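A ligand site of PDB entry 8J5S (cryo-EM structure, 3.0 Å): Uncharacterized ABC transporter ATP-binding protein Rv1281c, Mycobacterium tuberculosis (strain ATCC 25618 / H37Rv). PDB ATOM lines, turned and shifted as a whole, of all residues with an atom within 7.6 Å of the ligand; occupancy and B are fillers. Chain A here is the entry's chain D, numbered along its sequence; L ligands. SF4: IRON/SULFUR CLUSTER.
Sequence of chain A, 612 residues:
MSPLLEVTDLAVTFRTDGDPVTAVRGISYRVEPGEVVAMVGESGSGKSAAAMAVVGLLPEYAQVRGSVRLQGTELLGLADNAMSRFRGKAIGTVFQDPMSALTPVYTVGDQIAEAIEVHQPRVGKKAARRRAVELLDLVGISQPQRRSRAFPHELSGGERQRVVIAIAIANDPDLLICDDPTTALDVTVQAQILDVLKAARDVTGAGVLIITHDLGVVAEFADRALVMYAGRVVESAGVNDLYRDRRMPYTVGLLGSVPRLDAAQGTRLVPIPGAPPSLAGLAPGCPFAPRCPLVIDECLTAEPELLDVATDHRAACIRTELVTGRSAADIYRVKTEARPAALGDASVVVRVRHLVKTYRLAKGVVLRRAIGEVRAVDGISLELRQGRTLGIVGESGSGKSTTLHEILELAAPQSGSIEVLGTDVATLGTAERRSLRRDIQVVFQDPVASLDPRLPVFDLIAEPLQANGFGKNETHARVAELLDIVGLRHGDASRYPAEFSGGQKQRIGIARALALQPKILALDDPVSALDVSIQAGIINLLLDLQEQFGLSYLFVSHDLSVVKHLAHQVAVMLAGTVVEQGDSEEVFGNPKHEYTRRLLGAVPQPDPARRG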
ATOM      1  N   VAL A 234      12.750   0.498  28.664  1.00  0.00           N
ATOM      2  CA  VAL A 234      12.769  -0.737  27.822  1.00  0.00           C
ATOM      3  C   VAL A 234      13.592  -0.510  26.539  1.00  0.00           C
ATOM      4  O   VAL A 234      14.355  -1.427  26.176  1.00  0.00           O
ATOM      5  CB  VAL A 234      11.339  -1.218  27.518  1.00  0.00           C
ATOM      6  CG1 VAL A 234      11.307  -2.412  26.570  1.00  0.00           C
ATOM      7  CG2 VAL A 234      10.561  -1.518  28.788  1.00  0.00           C
ATOM      8  N   MET A 248      11.802  -4.662  19.271  1.00  0.00           N
ATOM      9  CA  MET A 248      11.566  -5.410  20.515  1.00  0.00           C
ATOM     10  C   MET A 248      10.091  -5.669  20.716  1.00  0.00           C
ATOM     11  O   MET A 248       9.276  -4.782  20.435  1.00  0.00           O
ATOM     12  CB  MET A 248      12.127  -4.645  21.716  1.00  0.00           C
ATOM     13  CG  MET A 248      11.367  -4.977  22.946  1.00  0.00           C
ATOM     14  SD  MET A 248      11.923  -4.311  24.475  1.00  0.00           S
ATOM     15  CE  MET A 248      10.635  -4.967  25.510  1.00  0.00           C
ATOM     16  N   PRO A 249       9.687  -6.845  21.242  1.00  0.00           N
ATOM     17  CA  PRO A 249       8.261  -7.196  21.278  1.00  0.00           C
ATOM     18  C   PRO A 249       7.339  -6.195  21.953  1.00  0.00           C
ATOM     19  O   PRO A 249       6.223  -5.970  21.447  1.00  0.00           O
ATOM     20  CB  PRO A 249       8.270  -8.532  22.016  1.00  0.00           C
ATOM     21  CG  PRO A 249       9.554  -9.126  21.668  1.00  0.00           C
ATOM     22  CD  PRO A 249      10.527  -8.000  21.572  1.00  0.00           C
ATOM     23  N   TYR A 250       7.731  -5.593  23.068  1.00  0.00           N
ATOM     24  CA  TYR A 250       6.813  -4.675  23.749  1.00  0.00           C
ATOM     25  C   TYR A 250       6.545  -3.438  22.904  1.00  0.00           C
ATOM     26  O   TYR A 250       5.402  -3.024  22.735  1.00  0.00           O
ATOM     27  CB  TYR A 250       7.372  -4.294  25.107  1.00  0.00           C
ATOM     28  CG  TYR A 250       6.578  -3.233  25.832  1.00  0.00           C
ATOM     29  CD1 TYR A 250       5.266  -3.432  26.162  1.00  0.00           C
ATOM     30  CD2 TYR A 250       7.170  -2.032  26.182  1.00  0.00           C
ATOM     31  CE1 TYR A 250       4.545  -2.469  26.822  1.00  0.00           C
ATOM     32  CE2 TYR A 250       6.458  -1.067  26.843  1.00  0.00           C
ATOM     33  CZ  TYR A 250       5.152  -1.290  27.161  1.00  0.00           C
ATOM     34  OH  TYR A 250       4.451  -0.323  27.822  1.00  0.00           O
ATOM     35  N   GLY A 285      13.282 -12.536  36.176  1.00  0.00           N
ATOM     36  CA  GLY A 285      13.202 -12.657  34.731  1.00  0.00           C
ATOM     37  C   GLY A 285      12.717 -11.377  34.109  1.00  0.00           C
ATOM     38  O   GLY A 285      12.457 -10.372  34.773  1.00  0.00           O
ATOM     39  N   CYS A 286      12.579 -11.392  32.780  1.00  0.00           N
ATOM     40  CA  CYS A 286      12.091 -10.223  32.056  1.00  0.00           C
ATOM     41  C   CYS A 286      10.650  -9.972  32.475  1.00  0.00           C
ATOM     42  O   CYS A 286       9.829 -10.892  32.480  1.00  0.00           O
ATOM     43  CB  CYS A 286      12.175 -10.438  30.546  1.00  0.00           C
ATOM     44  SG  CYS A 286      11.697  -9.003  29.566  1.00  0.00           S
ATOM     45  N   PRO A 287      10.336  -8.720  32.828  1.00  0.00           N
ATOM     46  CA  PRO A 287       8.965  -8.413  33.280  1.00  0.00           C
ATOM     47  C   PRO A 287       7.913  -8.668  32.230  1.00  0.00           C
ATOM     48  O   PRO A 287       6.738  -8.838  32.579  1.00  0.00           O
ATOM     49  CB  PRO A 287       9.046  -6.932  33.652  1.00  0.00           C
ATOM     50  CG  PRO A 287      10.470  -6.677  33.891  1.00  0.00           C
ATOM     51  CD  PRO A 287      11.215  -7.553  32.951  1.00  0.00           C
ATOM     52  N   PHE A 288       8.280  -8.681  30.956  1.00  0.00           N
ATOM     53  CA  PHE A 288       7.321  -8.929  29.884  1.00  0.00           C
ATOM     54  C   PHE A 288       7.109 -10.410  29.633  1.00  0.00           C
ATOM     55  O   PHE A 288       6.283 -10.750  28.789  1.00  0.00           O
ATOM     56  CB  PHE A 288       7.787  -8.255  28.598  1.00  0.00           C
ATOM     57  CG  PHE A 288       6.691  -7.961  27.637  1.00  0.00           C
ATOM     58  CD1 PHE A 288       5.546  -7.315  28.039  1.00  0.00           C
ATOM     59  CD2 PHE A 288       6.790  -8.332  26.319  1.00  0.00           C
ATOM     60  CE1 PHE A 288       4.541  -7.052  27.164  1.00  0.00           C
ATOM     61  CE2 PHE A 288       5.785  -8.071  25.434  1.00  0.00           C
ATOM     62  CZ  PHE A 288       4.661  -7.434  25.863  1.00  0.00           C
ATOM     63  N   ALA A 289       7.829 -11.274  30.330  1.00  0.00           N
ATOM     64  CA  ALA A 289       7.678 -12.712  30.115  1.00  0.00           C
ATOM     65  C   ALA A 289       6.240 -13.215  30.274  1.00  0.00           C
ATOM     66  O   ALA A 289       5.844 -14.103  29.507  1.00  0.00           O
ATOM     67  CB  ALA A 289       8.627 -13.470  31.040  1.00  0.00           C
ATOM     68  N   PRO A 290       5.433 -12.730  31.229  1.00  0.00           N
ATOM     69  CA  PRO A 290       4.032 -13.157  31.251  1.00  0.00           C
ATOM     70  C   PRO A 290       3.283 -12.913  29.959  1.00  0.00           C
ATOM     71  O   PRO A 290       2.454 -13.749  29.564  1.00  0.00           O
ATOM     72  CB  PRO A 290       3.444 -12.334  32.399  1.00  0.00           C
ATOM     73  CG  PRO A 290       4.565 -12.120  33.302  1.00  0.00           C
ATOM     74  CD  PRO A 290       5.800 -12.034  32.469  1.00  0.00           C
ATOM     75  N   ARG A 291       3.524 -11.794  29.283  1.00  0.00           N
ATOM     76  CA  ARG A 291       2.764 -11.416  28.104  1.00  0.00           C
ATOM     77  C   ARG A 291       3.538 -11.532  26.811  1.00  0.00           C
ATOM     78  O   ARG A 291       2.987 -11.230  25.749  1.00  0.00           O
ATOM     79  CB  ARG A 291       2.248  -9.987  28.256  1.00  0.00           C
ATOM     80  CG  ARG A 291       1.643  -9.698  29.599  1.00  0.00           C
ATOM     81  CD  ARG A 291       1.581  -8.234  29.863  1.00  0.00           C
ATOM     82  NE  ARG A 291       0.963  -7.495  28.764  1.00  0.00           N
ATOM     83  CZ  ARG A 291       0.459  -6.280  28.882  1.00  0.00           C
ATOM     84  NH1 ARG A 291       0.498  -5.661  30.052  1.00  0.00           N
ATOM     85  NH2 ARG A 291      -0.078  -5.676  27.849  1.00  0.00           N
ATOM     86  N   CYS A 292       4.823 -11.844  26.869  1.00  0.00           N
ATOM     87  CA  CYS A 292       5.589 -11.872  25.620  1.00  0.00           C
ATOM     88  C   CYS A 292       5.330 -13.083  24.755  1.00  0.00           C
ATOM     89  O   CYS A 292       5.414 -14.225  25.216  1.00  0.00           O
ATOM     90  CB  CYS A 292       7.077 -11.686  25.848  1.00  0.00           C
ATOM     91  SG  CYS A 292       7.938 -11.391  24.283  1.00  0.00           S
ATOM     92  N   PRO A 293       5.009 -12.841  23.477  1.00  0.00           N
ATOM     93  CA  PRO A 293       4.768 -13.966  22.575  1.00  0.00           C
ATOM     94  C   PRO A 293       6.006 -14.730  22.160  1.00  0.00           C
ATOM     95  O   PRO A 293       5.882 -15.735  21.456  1.00  0.00           O
ATOM     96  CB  PRO A 293       4.130 -13.293  21.358  1.00  0.00           C
ATOM     97  CG  PRO A 293       4.640 -11.914  21.394  1.00  0.00           C
ATOM     98  CD  PRO A 293       4.717 -11.549  22.833  1.00  0.00           C
ATOM     99  N   LEU A 294       7.186 -14.257  22.551  1.00  0.00           N
ATOM    100  CA  LEU A 294       8.425 -14.930  22.181  1.00  0.00           C
ATOM    101  C   LEU A 294       9.231 -15.351  23.400  1.00  0.00           C
ATOM    102  O   LEU A 294      10.447 -15.508  23.324  1.00  0.00           O
ATOM    103  CB  LEU A 294       9.273 -14.032  21.274  1.00  0.00           C
ATOM    104  CG  LEU A 294       8.586 -13.523  20.009  1.00  0.00           C
ATOM    105  CD1 LEU A 294       9.505 -12.571  19.253  1.00  0.00           C
ATOM    106  CD2 LEU A 294       8.167 -14.683  19.116  1.00  0.00           C
ATOM    107  N   VAL A 295       8.545 -15.540  24.518  1.00  0.00           N
ATOM    108  CA  VAL A 295       9.213 -15.934  25.754  1.00  0.00           C
ATOM    109  C   VAL A 295       9.831 -17.324  25.634  1.00  0.00           C
ATOM    110  O   VAL A 295       9.213 -18.259  25.108  1.00  0.00           O
ATOM    111  CB  VAL A 295       8.240 -15.916  26.947  1.00  0.00           C
ATOM    112  CG1 VAL A 295       7.149 -16.965  26.768  1.00  0.00           C
ATOM    113  CG2 VAL A 295       8.993 -16.134  28.252  1.00  0.00           C
ATOM    114  N   ILE A 296      11.054 -17.454  26.122  1.00  0.00           N
ATOM    115  CA  ILE A 296      11.782 -18.716  26.134  1.00  0.00           C
ATOM    116  C   ILE A 296      12.257 -18.967  27.562  1.00  0.00           C
ATOM    117  O   ILE A 296      12.335 -18.024  28.355  1.00  0.00           O
ATOM    118  CB  ILE A 296      12.995 -18.688  25.180  1.00  0.00           C
ATOM    119  CG1 ILE A 296      13.944 -17.556  25.567  1.00  0.00           C
ATOM    120  CG2 ILE A 296      12.528 -18.535  23.743  1.00  0.00           C
ATOM    121  CD1 ILE A 296      15.136 -17.425  24.640  1.00  0.00           C
ATOM    122  N   GLU A 298      14.909 -19.022  28.690  1.00  0.00           N
ATOM    123  CA  GLU A 298      16.044 -18.163  29.011  1.00  0.00           C
ATOM    124  C   GLU A 298      15.648 -16.758  29.409  1.00  0.00           C
ATOM    125  O   GLU A 298      16.405 -16.095  30.106  1.00  0.00           O
ATOM    126  CB  GLU A 298      17.022 -18.099  27.834  1.00  0.00           C
ATOM    127  CG  GLU A 298      17.935 -19.311  27.694  1.00  0.00           C
ATOM    128  CD  GLU A 298      18.732 -19.637  28.944  1.00  0.00           C
ATOM    129  OE1 GLU A 298      19.493 -20.624  28.934  1.00  0.00           O
ATOM    130  OE2 GLU A 298      18.632 -18.916  29.946  1.00  0.00           O
ATOM    131  N   CYS A 299      14.444 -16.377  29.021  1.00  0.00           N
ATOM    132  CA  CYS A 299      13.920 -15.064  29.305  1.00  0.00           C
ATOM    133  C   CYS A 299      13.427 -14.927  30.745  1.00  0.00           C
ATOM    134  O   CYS A 299      12.803 -13.933  31.111  1.00  0.00           O
ATOM    135  CB  CYS A 299      12.765 -14.841  28.349  1.00  0.00           C
ATOM    136  SG  CYS A 299      13.203 -15.007  26.605  1.00  0.00           S
ATOM    137  N   LEU A 300      13.721 -15.951  31.544  1.00  0.00           N
ATOM    138  CA  LEU A 300      13.332 -15.982  32.947  1.00  0.00           C
ATOM    139  C   LEU A 300      14.493 -16.229  33.890  1.00  0.00           C
ATOM    140  O   LEU A 300      14.288 -16.297  35.106  1.00  0.00           O
ATOM    141  CB  LEU A 300      12.258 -17.054  33.181  1.00  0.00           C
ATOM    142  CG  LEU A 300      11.064 -17.064  32.223  1.00  0.00           C
ATOM    143  CD1 LEU A 300      11.294 -17.997  31.075  1.00  0.00           C
ATOM    144  CD2 LEU A 300       9.802 -17.467  32.955  1.00  0.00           C
ATOM    145  N   ALA A 302      17.179 -14.116  34.128  1.00  0.00           N
ATOM    146  CA  ALA A 302      17.514 -12.811  34.675  1.00  0.00           C
ATOM    147  C   ALA A 302      16.859 -11.745  33.825  1.00  0.00           C
ATOM    148  O   ALA A 302      16.445 -11.994  32.686  1.00  0.00           O
ATOM    149  CB  ALA A 302      19.030 -12.597  34.728  1.00  0.00           C
ATOM    150  N   GLU A 303      16.775 -10.545  34.384  1.00  0.00           N
ATOM    151  CA  GLU A 303      16.292  -9.394  33.635  1.00  0.00           C
ATOM    152  C   GLU A 303      17.347  -8.980  32.628  1.00  0.00           C
ATOM    153  O   GLU A 303      18.495  -8.726  33.022  1.00  0.00           O
ATOM    154  CB  GLU A 303      15.996  -8.244  34.575  1.00  0.00           C
ATOM    155  CG  GLU A 303      14.887  -7.349  34.115  1.00  0.00           C
ATOM    156  CD  GLU A 303      14.561  -6.293  35.136  1.00  0.00           C
ATOM    157  OE1 GLU A 303      13.387  -5.856  35.200  1.00  0.00           O
ATOM    158  OE2 GLU A 303      15.466  -5.898  35.887  1.00  0.00           O
ATOM    159  N   PRO A 304      17.025  -8.903  31.341  1.00  0.00           N
ATOM    160  CA  PRO A 304      18.001  -8.403  30.370  1.00  0.00           C
ATOM    161  C   PRO A 304      18.248  -6.926  30.562  1.00  0.00           C
ATOM    162  O   PRO A 304      17.451  -6.186  31.138  1.00  0.00           O
ATOM    163  CB  PRO A 304      17.342  -8.687  29.030  1.00  0.00           C
ATOM    164  CG  PRO A 304      15.904  -8.735  29.325  1.00  0.00           C
ATOM    165  CD  PRO A 304      15.769  -9.312  30.707  1.00  0.00           C
ATOM    166  N   ALA A 316      16.118  -3.803  25.661  1.00  0.00           N
ATOM    167  CA  ALA A 316      16.292  -4.739  26.766  1.00  0.00           C
ATOM    168  C   ALA A 316      15.667  -6.087  26.407  1.00  0.00           C
ATOM    169  O   ALA A 316      14.612  -6.475  26.907  1.00  0.00           O
ATOM    170  CB  ALA A 316      15.709  -4.157  28.047  1.00  0.00           C
ATOM    171  N   CYS A 317      16.315  -6.771  25.476  1.00  0.00           N
ATOM    172  CA  CYS A 317      15.849  -8.057  25.011  1.00  0.00           C
ATOM    173  C   CYS A 317      17.031  -8.905  24.595  1.00  0.00           C
ATOM    174  O   CYS A 317      18.084  -8.388  24.222  1.00  0.00           O
ATOM    175  CB  CYS A 317      14.881  -7.884  23.830  1.00  0.00           C
ATOM    176  SG  CYS A 317      14.178  -9.433  23.209  1.00  0.00           S
ATOM    177  N   ILE A 318      16.849 -10.220  24.654  1.00  0.00           N
ATOM    178  CA  ILE A 318      17.899 -11.152  24.302  1.00  0.00           C
ATOM    179  C   ILE A 318      17.684 -11.729  22.905  1.00  0.00           C
ATOM    180  O   ILE A 318      18.646 -11.846  22.135  1.00  0.00           O
ATOM    181  CB  ILE A 318      18.021 -12.278  25.347  1.00  0.00           C
ATOM    182  CG1 ILE A 318      16.668 -12.873  25.695  1.00  0.00           C
ATOM    183  CG2 ILE A 318      18.672 -11.756  26.607  1.00  0.00           C
ATOM    184  CD1 ILE A 318      16.795 -14.178  26.407  1.00  0.00           C
ATOM    185  N   ARG A 319      16.442 -12.045  22.561  1.00  0.00           N
ATOM    186  CA  ARG A 319      16.132 -12.576  21.242  1.00  0.00           C
ATOM    187  C   ARG A 319      15.574 -11.464  20.357  1.00  0.00           C
ATOM    188  O   ARG A 319      14.501 -11.614  19.769  1.00  0.00           O
ATOM    189  CB  ARG A 319      15.120 -13.723  21.360  1.00  0.00           C
ATOM    190  CG  ARG A 319      13.791 -13.326  21.990  1.00  0.00           C
ATOM    191  CD  ARG A 319      12.917 -14.549  22.226  1.00  0.00           C
ATOM    192  NE  ARG A 319      12.716 -15.326  21.013  1.00  0.00           N
ATOM    193  CZ  ARG A 319      13.478 -16.350  20.654  1.00  0.00           C
ATOM    194  NH1 ARG A 319      14.493 -16.729  21.409  1.00  0.00           N
ATOM    195  NH2 ARG A 319      13.219 -17.011  19.522  1.00  0.00           N
ATOM    196  N   THR A 320      16.307 -10.364  20.261  1.00  0.00           N
ATOM    197  CA  THR A 320      15.883  -9.236  19.452  1.00  0.00           C
ATOM    198  C   THR A 320      16.296  -9.378  18.004  1.00  0.00           C
ATOM    199  O   THR A 320      16.098  -8.439  17.223  1.00  0.00           O
ATOM    200  CB  THR A 320      16.453  -7.940  20.022  1.00  0.00           C
ATOM    201  OG1 THR A 320      15.825  -6.824  19.393  1.00  0.00           O
ATOM    202  CG2 THR A 320      17.938  -7.889  19.775  1.00  0.00           C
ATOM    203  N   VAL A 323      12.965 -10.003  15.696  1.00  0.00           N
ATOM    204  CA  VAL A 323      11.975  -8.949  15.602  1.00  0.00           C
ATOM    205  C   VAL A 323      12.182  -8.055  14.391  1.00  0.00           C
ATOM    206  O   VAL A 323      11.207  -7.486  13.886  1.00  0.00           O
ATOM    207  CB  VAL A 323      11.937  -8.118  16.894  1.00  0.00           C
ATOM    208  CG1 VAL A 323      11.009  -6.954  16.782  1.00  0.00           C
ATOM    209  CG2 VAL A 323      11.515  -8.991  18.049  1.00  0.00           C
HETATM  210 FE1  SF4 L   1      12.381 -12.685  26.327  1.00  0.00          FE
HETATM  211 FE2  SF4 L   1      12.533 -10.314  24.983  1.00  0.00          FE
HETATM  212 FE3  SF4 L   1      11.523 -10.390  27.518  1.00  0.00          FE
HETATM  213 FE4  SF4 L   1      10.125 -11.478  25.434  1.00  0.00          FE
HETATM  214  S1  SF4 L   1      10.651  -9.278  25.733  1.00  0.00           S
HETATM  215  S2  SF4 L   1      10.455 -12.400  27.489  1.00  0.00           S
HETATM  216  S3  SF4 L   1      11.800 -12.299  24.172  1.00  0.00           S
HETATM  217  S4  SF4 L   1      13.662 -10.871  26.894  1.00  0.00           S
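The backbone carbonyl oxygen (O) of Leu 294 lies close to a sulfur (S3) of the ligand, at 3.6 Å. Merely in contact with the ligand: Ala 289, Pro 304, Ile 318 and Arg 319. Hydrophobic or aromatic side chains within 4 Å of the ligand: Pro 304 and Ile 318. Nine residues have an atom within 4 Å of the ligand: Cys 286, Ala 289, Cys 292, Leu 294, Cys 299, Pro 304, Cys 317, Ile 318 and Arg 319. The nearest printed residue that does not touch the ligand is Phe 288 (4.02 Å).
FE4 of the ligand is bound by SG of Cys 292. The side-chain sulfur (SG) of Cys 299 binds an iron atom (FE1) of the ligand (2.5 Å). An iron atom (FE3) of the ligand is bound by the side-chain sulfur (SG) of Cys 286, 2.5 Å away. FE2 of the ligand is bound by SG of Cys 317 (2.6 Å).
The side-chain sulfur of Cys 292 sits close to the backbone NH of Leu 294. The backbone NH of Cys 286 lies within hydrogen-bond range of the backbone carbonyl oxygen of Cys 299 (3.0 Å). The side-chain sulfur (SG) of Cys 299 sits close to the backbone NH (N) of Ile 296 (3.3 Å). The side-chain sulfur (SG) of Cys 286 lies close to the backbone NH (N) of Phe 288. The side-chain sulfur of Cys 317 lies close to the backbone NH of Arg 319 (3.5 Å). SG of Cys 317 lies close to N of Thr 320, at 3.8 Å. The guanidinium group (NE) of Arg 319 sits close to the backbone carbonyl oxygen (O) of Leu 294.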
